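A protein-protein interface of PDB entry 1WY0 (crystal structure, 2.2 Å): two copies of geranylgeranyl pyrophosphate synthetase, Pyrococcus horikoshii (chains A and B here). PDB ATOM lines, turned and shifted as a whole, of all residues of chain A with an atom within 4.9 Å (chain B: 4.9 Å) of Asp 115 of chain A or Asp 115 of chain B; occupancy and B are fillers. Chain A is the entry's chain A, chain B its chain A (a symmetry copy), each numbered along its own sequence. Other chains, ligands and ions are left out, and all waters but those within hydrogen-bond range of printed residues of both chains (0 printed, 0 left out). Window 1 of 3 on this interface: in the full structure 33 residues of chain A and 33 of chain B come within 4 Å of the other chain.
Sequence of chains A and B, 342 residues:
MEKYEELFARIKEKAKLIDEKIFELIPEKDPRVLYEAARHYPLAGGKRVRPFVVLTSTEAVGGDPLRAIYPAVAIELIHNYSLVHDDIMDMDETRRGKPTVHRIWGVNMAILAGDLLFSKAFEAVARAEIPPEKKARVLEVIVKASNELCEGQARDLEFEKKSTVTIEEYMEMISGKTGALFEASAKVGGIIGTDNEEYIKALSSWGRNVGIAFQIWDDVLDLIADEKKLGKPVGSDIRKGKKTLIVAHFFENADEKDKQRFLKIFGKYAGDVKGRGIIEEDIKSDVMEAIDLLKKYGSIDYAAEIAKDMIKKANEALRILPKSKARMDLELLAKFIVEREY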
ATOM      1  N   TYR A  81       7.008  11.870  -0.181  1.00  0.00           N
ATOM      2  CA  TYR A  81       7.779  12.399   0.934  1.00  0.00           C
ATOM      3  C   TYR A  81       8.312  13.797   0.595  1.00  0.00           C
ATOM      4  O   TYR A  81       8.429  14.651   1.483  1.00  0.00           O
ATOM      5  CB  TYR A  81       8.945  11.456   1.278  1.00  0.00           C
ATOM      6  CG  TYR A  81      10.323  12.063   1.133  1.00  0.00           C
ATOM      7  CD1 TYR A  81      11.070  11.880  -0.030  1.00  0.00           C
ATOM      8  CD2 TYR A  81      10.902  12.786   2.179  1.00  0.00           C
ATOM      9  CE1 TYR A  81      12.357  12.391  -0.148  1.00  0.00           C
ATOM     10  CE2 TYR A  81      12.194  13.308   2.069  1.00  0.00           C
ATOM     11  CZ  TYR A  81      12.917  13.103   0.908  1.00  0.00           C
ATOM     12  OH  TYR A  81      14.211  13.566   0.817  1.00  0.00           O
ATOM     13  N   HIS A  85       7.638  17.366   2.956  1.00  0.00           N
ATOM     14  CA  HIS A  85       8.711  18.220   3.454  1.00  0.00           C
ATOM     15  C   HIS A  85       8.721  19.586   2.764  1.00  0.00           C
ATOM     16  O   HIS A  85       8.967  20.623   3.367  1.00  0.00           O
ATOM     17  CB  HIS A  85      10.040  17.504   3.211  1.00  0.00           C
ATOM     18  CG  HIS A  85      10.280  16.501   4.308  1.00  0.00           C
ATOM     19  ND1 HIS A  85      11.439  15.809   4.443  1.00  0.00           N
ATOM     20  CD2 HIS A  85       9.415  16.124   5.341  1.00  0.00           C
ATOM     21  CE1 HIS A  85      11.275  15.037   5.535  1.00  0.00           C
ATOM     22  NE2 HIS A  85      10.073  15.205   6.092  1.00  0.00           N
ATOM     23  N   ILE A 111       7.468  16.176   9.521  1.00  0.00           N
ATOM     24  CA  ILE A 111       8.833  15.830   9.175  1.00  0.00           C
ATOM     25  C   ILE A 111       8.942  14.311   9.265  1.00  0.00           C
ATOM     26  O   ILE A 111       9.400  13.656   8.316  1.00  0.00           O
ATOM     27  CB  ILE A 111       9.825  16.458  10.143  1.00  0.00           C
ATOM     28  CG1 ILE A 111       9.951  17.947   9.861  1.00  0.00           C
ATOM     29  CG2 ILE A 111      11.171  15.772  10.023  1.00  0.00           C
ATOM     30  CD1 ILE A 111      10.742  18.738  10.951  1.00  0.00           C
ATOM     31  N   LEU A 112       8.515  13.753  10.401  1.00  0.00           N
ATOM     32  CA  LEU A 112       8.557  12.305  10.593  1.00  0.00           C
ATOM     33  C   LEU A 112       7.774  11.525   9.537  1.00  0.00           C
ATOM     34  O   LEU A 112       8.204  10.451   9.142  1.00  0.00           O
ATOM     35  CB  LEU A 112       8.028  11.921  11.973  1.00  0.00           C
ATOM     36  CG  LEU A 112       9.021  12.108  13.117  1.00  0.00           C
ATOM     37  CD1 LEU A 112       8.403  11.568  14.375  1.00  0.00           C
ATOM     38  CD2 LEU A 112      10.353  11.372  12.806  1.00  0.00           C
ATOM     39  N   ALA A 113       6.623  12.048   9.096  1.00  0.00           N
ATOM     40  CA  ALA A 113       5.829  11.365   8.083  1.00  0.00           C
ATOM     41  C   ALA A 113       6.630  11.318   6.783  1.00  0.00           C
ATOM     42  O   ALA A 113       6.662  10.292   6.103  1.00  0.00           O
ATOM     43  CB  ALA A 113       4.512  12.091   7.859  1.00  0.00           C
ATOM     44  N   GLY A 114       7.254  12.442   6.433  1.00  0.00           N
ATOM     45  CA  GLY A 114       8.085  12.489   5.245  1.00  0.00           C
ATOM     46  C   GLY A 114       9.202  11.470   5.391  1.00  0.00           C
ATOM     47  O   GLY A 114       9.509  10.768   4.445  1.00  0.00           O
ATOM     48  N   ASP A 115       9.804  11.374   6.573  1.00  0.00           N
ATOM     49  CA  ASP A 115      10.887  10.415   6.809  1.00  0.00           C
ATOM     50  C   ASP A 115      10.416   8.981   6.637  1.00  0.00           C
ATOM     51  O   ASP A 115      11.120   8.148   6.066  1.00  0.00           O
ATOM     52  CB  ASP A 115      11.473  10.562   8.229  1.00  0.00           C
ATOM     53  CG  ASP A 115      12.284  11.835   8.391  1.00  0.00           C
ATOM     54  OD1 ASP A 115      12.592  12.475   7.344  1.00  0.00           O
ATOM     55  OD2 ASP A 115      12.622  12.177   9.550  1.00  0.00           O
ATOM     56  N   LEU A 116       9.237   8.687   7.157  1.00  0.00           N
ATOM     57  CA  LEU A 116       8.692   7.343   7.060  1.00  0.00           C
ATOM     58  C   LEU A 116       8.437   7.006   5.598  1.00  0.00           C
ATOM     59  O   LEU A 116       8.725   5.906   5.141  1.00  0.00           O
ATOM     60  CB  LEU A 116       7.376   7.219   7.837  1.00  0.00           C
ATOM     61  CG  LEU A 116       6.792   5.813   7.602  1.00  0.00           C
ATOM     62  CD1 LEU A 116       7.729   4.791   8.220  1.00  0.00           C
ATOM     63  CD2 LEU A 116       5.413   5.693   8.181  1.00  0.00           C
ATOM     64  N   LEU A 117       7.858   7.948   4.877  1.00  0.00           N
ATOM     65  CA  LEU A 117       7.593   7.753   3.460  1.00  0.00           C
ATOM     66  C   LEU A 117       8.887   7.465   2.696  1.00  0.00           C
ATOM     67  O   LEU A 117       8.906   6.599   1.827  1.00  0.00           O
ATOM     68  CB  LEU A 117       6.902   8.991   2.879  1.00  0.00           C
ATOM     69  CG  LEU A 117       5.392   9.065   3.103  1.00  0.00           C
ATOM     70  CD1 LEU A 117       4.867  10.447   2.683  1.00  0.00           C
ATOM     71  CD2 LEU A 117       4.704   7.945   2.312  1.00  0.00           C
ATOM     72  N   PHE A 118       9.957   8.187   3.019  1.00  0.00           N
ATOM     73  CA  PHE A 118      11.255   7.998   2.339  1.00  0.00           C
ATOM     74  C   PHE A 118      11.809   6.602   2.653  1.00  0.00           C
ATOM     75  O   PHE A 118      12.264   5.882   1.763  1.00  0.00           O
ATOM     76  CB  PHE A 118      12.271   9.069   2.785  1.00  0.00           C
ATOM     77  CG  PHE A 118      13.464   9.206   1.859  1.00  0.00           C
ATOM     78  CD1 PHE A 118      13.366   8.859   0.532  1.00  0.00           C
ATOM     79  CD2 PHE A 118      14.685   9.688   2.318  1.00  0.00           C
ATOM     80  CE1 PHE A 118      14.444   8.982  -0.330  1.00  0.00           C
ATOM     81  CE2 PHE A 118      15.786   9.817   1.442  1.00  0.00           C
ATOM     82  CZ  PHE A 118      15.650   9.461   0.120  1.00  0.00           C
ATOM     83  N   SER A 119      11.779   6.243   3.926  1.00  0.00           N
ATOM     84  CA  SER A 119      12.229   4.941   4.382  1.00  0.00           C
ATOM     85  C   SER A 119      11.423   3.830   3.680  1.00  0.00           C
ATOM     86  O   SER A 119      11.970   2.796   3.299  1.00  0.00           O
ATOM     87  CB  SER A 119      12.028   4.846   5.898  1.00  0.00           C
ATOM     88  OG  SER A 119      12.414   3.575   6.393  1.00  0.00           O
ATOM     89  N   CYS A 150      17.206  16.580  -3.357  1.00  0.00           N
ATOM     90  CA  CYS A 150      17.549  17.404  -2.193  1.00  0.00           C
ATOM     91  C   CYS A 150      18.390  18.607  -2.648  1.00  0.00           C
ATOM     92  O   CYS A 150      18.242  19.716  -2.143  1.00  0.00           O
ATOM     93  CB  CYS A 150      18.369  16.608  -1.160  1.00  0.00           C
ATOM     94  SG  CYS A 150      17.554  15.221  -0.320  1.00  0.00           S
ATOM     95  N   TYR B  81      21.432  11.783  10.541  1.00  0.00           N
ATOM     96  CA  TYR B  81      20.222  12.407  10.024  1.00  0.00           C
ATOM     97  C   TYR B  81      19.141  12.450  11.112  1.00  0.00           C
ATOM     98  O   TYR B  81      18.341  13.392  11.157  1.00  0.00           O
ATOM     99  CB  TYR B  81      19.706  11.642   8.793  1.00  0.00           C
ATOM    100  CG  TYR B  81      18.323  11.046   8.944  1.00  0.00           C
ATOM    101  CD1 TYR B  81      18.152   9.714   9.320  1.00  0.00           C
ATOM    102  CD2 TYR B  81      17.182  11.803   8.666  1.00  0.00           C
ATOM    103  CE1 TYR B  81      16.886   9.147   9.409  1.00  0.00           C
ATOM    104  CE2 TYR B  81      15.904  11.244   8.757  1.00  0.00           C
ATOM    105  CZ  TYR B  81      15.763   9.917   9.123  1.00  0.00           C
ATOM    106  OH  TYR B  81      14.509   9.346   9.158  1.00  0.00           O
ATOM    107  N   HIS B  85      17.099  16.024  12.462  1.00  0.00           N
ATOM    108  CA  HIS B  85      15.648  16.166  12.482  1.00  0.00           C
ATOM    109  C   HIS B  85      15.098  16.219  13.910  1.00  0.00           C
ATOM    110  O   HIS B  85      14.177  16.960  14.230  1.00  0.00           O
ATOM    111  CB  HIS B  85      15.043  14.977  11.735  1.00  0.00           C
ATOM    112  CG  HIS B  85      15.085  15.239  10.253  1.00  0.00           C
ATOM    113  ND1 HIS B  85      14.497  14.429   9.337  1.00  0.00           N
ATOM    114  CD2 HIS B  85      15.687  16.307   9.579  1.00  0.00           C
ATOM    115  CE1 HIS B  85      14.737  14.999   8.141  1.00  0.00           C
ATOM    116  NE2 HIS B  85      15.448  16.124   8.255  1.00  0.00           N
ATOM    117  N   ILE B 111      16.042  20.446   7.576  1.00  0.00           N
ATOM    118  CA  ILE B 111      15.238  19.315   7.155  1.00  0.00           C
ATOM    119  C   ILE B 111      15.942  18.693   5.953  1.00  0.00           C
ATOM    120  O   ILE B 111      16.195  17.478   5.931  1.00  0.00           O
ATOM    121  CB  ILE B 111      13.840  19.753   6.741  1.00  0.00           C
ATOM    122  CG1 ILE B 111      13.019  20.094   7.974  1.00  0.00           C
ATOM    123  CG2 ILE B 111      13.172  18.657   5.935  1.00  0.00           C
ATOM    124  CD1 ILE B 111      11.659  20.797   7.661  1.00  0.00           C
ATOM    125  N   LEU B 112      16.265  19.526   4.960  1.00  0.00           N
ATOM    126  CA  LEU B 112      16.956  19.046   3.766  1.00  0.00           C
ATOM    127  C   LEU B 112      18.294  18.368   4.064  1.00  0.00           C
ATOM    128  O   LEU B 112      18.639  17.402   3.400  1.00  0.00           O
ATOM    129  CB  LEU B 112      17.197  20.185   2.778  1.00  0.00           C
ATOM    130  CG  LEU B 112      15.988  20.568   1.931  1.00  0.00           C
ATOM    131  CD1 LEU B 112      16.418  21.601   0.929  1.00  0.00           C
ATOM    132  CD2 LEU B 112      15.411  19.320   1.210  1.00  0.00           C
ATOM    133  N   ALA B 113      19.051  18.879   5.043  1.00  0.00           N
ATOM    134  CA  ALA B 113      20.333  18.279   5.389  1.00  0.00           C
ATOM    135  C   ALA B 113      20.084  16.873   5.934  1.00  0.00           C
ATOM    136  O   ALA B 113      20.800  15.932   5.592  1.00  0.00           O
ATOM    137  CB  ALA B 113      21.053  19.122   6.428  1.00  0.00           C
ATOM    138  N   GLY B 114      19.081  16.746   6.803  1.00  0.00           N
ATOM    139  CA  GLY B 114      18.727  15.447   7.339  1.00  0.00           C
ATOM    140  C   GLY B 114      18.345  14.531   6.189  1.00  0.00           C
ATOM    141  O   GLY B 114      18.742  13.381   6.172  1.00  0.00           O
ATOM    142  N   ASP B 115      17.587  15.036   5.219  1.00  0.00           N
ATOM    143  CA  ASP B 115      17.175  14.231   4.066  1.00  0.00           C
ATOM    144  C   ASP B 115      18.369  13.764   3.251  1.00  0.00           C
ATOM    145  O   ASP B 115      18.416  12.621   2.795  1.00  0.00           O
ATOM    146  CB  ASP B 115      16.233  15.020   3.133  1.00  0.00           C
ATOM    147  CG  ASP B 115      14.858  15.230   3.741  1.00  0.00           C
ATOM    148  OD1 ASP B 115      14.562  14.561   4.773  1.00  0.00           O
ATOM    149  OD2 ASP B 115      14.082  16.041   3.181  1.00  0.00           O
ATOM    150  N   LEU B 116      19.320  14.658   3.042  1.00  0.00           N
ATOM    151  CA  LEU B 116      20.503  14.323   2.267  1.00  0.00           C
ATOM    152  C   LEU B 116      21.295  13.247   2.995  1.00  0.00           C
ATOM    153  O   LEU B 116      21.785  12.301   2.389  1.00  0.00           O
ATOM    154  CB  LEU B 116      21.399  15.550   2.063  1.00  0.00           C
ATOM    155  CG  LEU B 116      22.685  15.110   1.339  1.00  0.00           C
ATOM    156  CD1 LEU B 116      22.316  14.637  -0.056  1.00  0.00           C
ATOM    157  CD2 LEU B 116      23.686  16.227   1.278  1.00  0.00           C
ATOM    158  N   LEU B 117      21.451  13.418   4.294  1.00  0.00           N
ATOM    159  CA  LEU B 117      22.163  12.439   5.101  1.00  0.00           C
ATOM    160  C   LEU B 117      21.501  11.063   5.001  1.00  0.00           C
ATOM    161  O   LEU B 117      22.194  10.056   4.897  1.00  0.00           O
ATOM    162  CB  LEU B 117      22.209  12.896   6.563  1.00  0.00           C
ATOM    163  CG  LEU B 117      23.308  13.903   6.901  1.00  0.00           C
ATOM    164  CD1 LEU B 117      23.100  14.449   8.322  1.00  0.00           C
ATOM    165  CD2 LEU B 117      24.678  13.228   6.759  1.00  0.00           C
ATOM    166  N   PHE B 118      20.171  11.024   5.033  1.00  0.00           N
ATOM    167  CA  PHE B 118      19.430   9.749   4.952  1.00  0.00           C
ATOM    168  C   PHE B 118      19.652   9.103   3.577  1.00  0.00           C
ATOM    169  O   PHE B 118      19.925   7.907   3.471  1.00  0.00           O
ATOM    170  CB  PHE B 118      17.921   9.973   5.178  1.00  0.00           C
ATOM    171  CG  PHE B 118      17.157   8.708   5.519  1.00  0.00           C
ATOM    172  CD1 PHE B 118      17.792   7.643   6.112  1.00  0.00           C
ATOM    173  CD2 PHE B 118      15.798   8.589   5.248  1.00  0.00           C
ATOM    174  CE1 PHE B 118      17.109   6.480   6.435  1.00  0.00           C
ATOM    175  CE2 PHE B 118      15.098   7.407   5.577  1.00  0.00           C
ATOM    176  CZ  PHE B 118      15.766   6.361   6.171  1.00  0.00           C
ATOM    177  N   SER B 119      19.513   9.906   2.535  1.00  0.00           N
ATOM    178  CA  SER B 119      19.728   9.461   1.171  1.00  0.00           C
ATOM    179  C   SER B 119      21.162   8.918   1.013  1.00  0.00           C
ATOM    180  O   SER B 119      21.389   7.916   0.337  1.00  0.00           O
ATOM    181  CB  SER B 119      19.515  10.642   0.219  1.00  0.00           C
ATOM    182  OG  SER B 119      19.753  10.273  -1.128  1.00  0.00           O
ATOM    183  N   CYS B 150      11.673   5.918  13.116  1.00  0.00           N
ATOM    184  CA  CYS B 150      10.632   6.930  12.906  1.00  0.00           C
ATOM    185  C   CYS B 150       9.443   6.641  13.836  1.00  0.00           C
ATOM    186  O   CYS B 150       8.823   7.551  14.379  1.00  0.00           O
ATOM    187  CB  CYS B 150      10.119   6.918  11.454  1.00  0.00           C
ATOM    188  SG  CYS B 150      11.278   7.399  10.143  1.00  0.00           S
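The side-chain carboxylate of Asp 115 of chain B sits close to the side-chain hydroxyl of Tyr 81 of chain A, 3.4 Å away.
The side-chain carboxylate (OD2) of Asp 115 of chain B sits at hydrogen-bond distance from a ring nitrogen (ND1) of His 85 of chain A, at 2.9 Å.
The side-chain carboxylate (OD2) of Asp 115 of chain A lies close to the side-chain hydroxyl (OH) of Tyr 81 of chain B (3.4 Å).
The side-chain carboxylate (OD2) of Asp 115 of chain A lies within hydrogen-bond range of a ring nitrogen (ND1) of His 85 of chain B.
O of Ile 111 of chain A sits at hydrogen-bond distance from NE2 of His 85 of chain A (2.8 Å).
NE2 of His 85 of chain B is in hydrogen-bond range of O of Ile 111 of chain B, 2.8 Å away.
Among the printed residues, pairs that only touch across the chains: His 85 of chain A with Ile 111 of chain B, Ile 111 of chain A with His 85 of chain B, Ile 111 of chain A with Ile 111 of chain B, Asp 115 of chain A with Asp 115 of chain B, Asp 115 of chain A with Cys 150 of chain B, Leu 116 of chain A with Cys 150 of chain B, Phe 118 of chain A with Phe 118 of chain B, Phe 118 of chain A with Ser 119 of chain B, Ser 119 of chain A with Phe 118 of chain B, Cys 150 of chain A with Asp 115 of chain B and Cys 150 of chain A with Leu 116 of chain B.
Printed residues of chain A within 4 Å of Asp 115 of chain B: Tyr 81, His 85, Asp 115 and Cys 150.
Of the printed residues of chain A, Cys 150 of chain B touches Asp 115 and Leu 116.
Printed residues of chain A within 4 Å of Ser 119 of chain B: Phe 118.
Of the printed residues of chain B, Cys 150 of chain A touches Asp 115 and Leu 116.
Printed residues of chain B within 4 Å of Ser 119 of chain A: Phe 118.
Leu 117 of chain A touches none of the printed residues of chain B.
Gly 114 of chain B touches none of the printed residues of chain A.
The nearest residue of chain B that does not touch Asp 115 of chain A is Phe 118 of chain B (4.1 Å).
The nearest residue of chain A that does not touch Asp 115 of chain B is Phe 118 of chain A (4.1 Å).
Of the 12 printed residues of chain A, 8 touch a printed residue of chain B.
Along chain A the printed residues that touch a printed residue of chain B span positions 81 to 150.
Of the 12 printed residues of chain B, 8 touch a printed residue of chain A.
Hydrophobic or aromatic side chains of chain B within 4 Å of the printed part of chain A: Tyr 81, His 85, Ile 111 and Phe 118.
Among the printed residues, 15 pairs touch across the chains.
Tyr 81 of chain A touches Asp 115 of chain B, and with the chains exchanged Asp 115 of chain A touches Tyr 81 of chain B.
His 85 of chain A touches Ile 111 of chain B, and with the chains exchanged Ile 111 of chain A touches His 85 of chain B.
His 85 of chain A touches Asp 115 of chain B, and with the chains exchanged Asp 115 of chain A touches His 85 of chain B.
Asp 115 of chain A touches its own counterpart, Asp 115 of chain B.
Of the 15 pairs that touch across the chains among the printed residues, 15 have their exchanged pair printed and touching as well.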
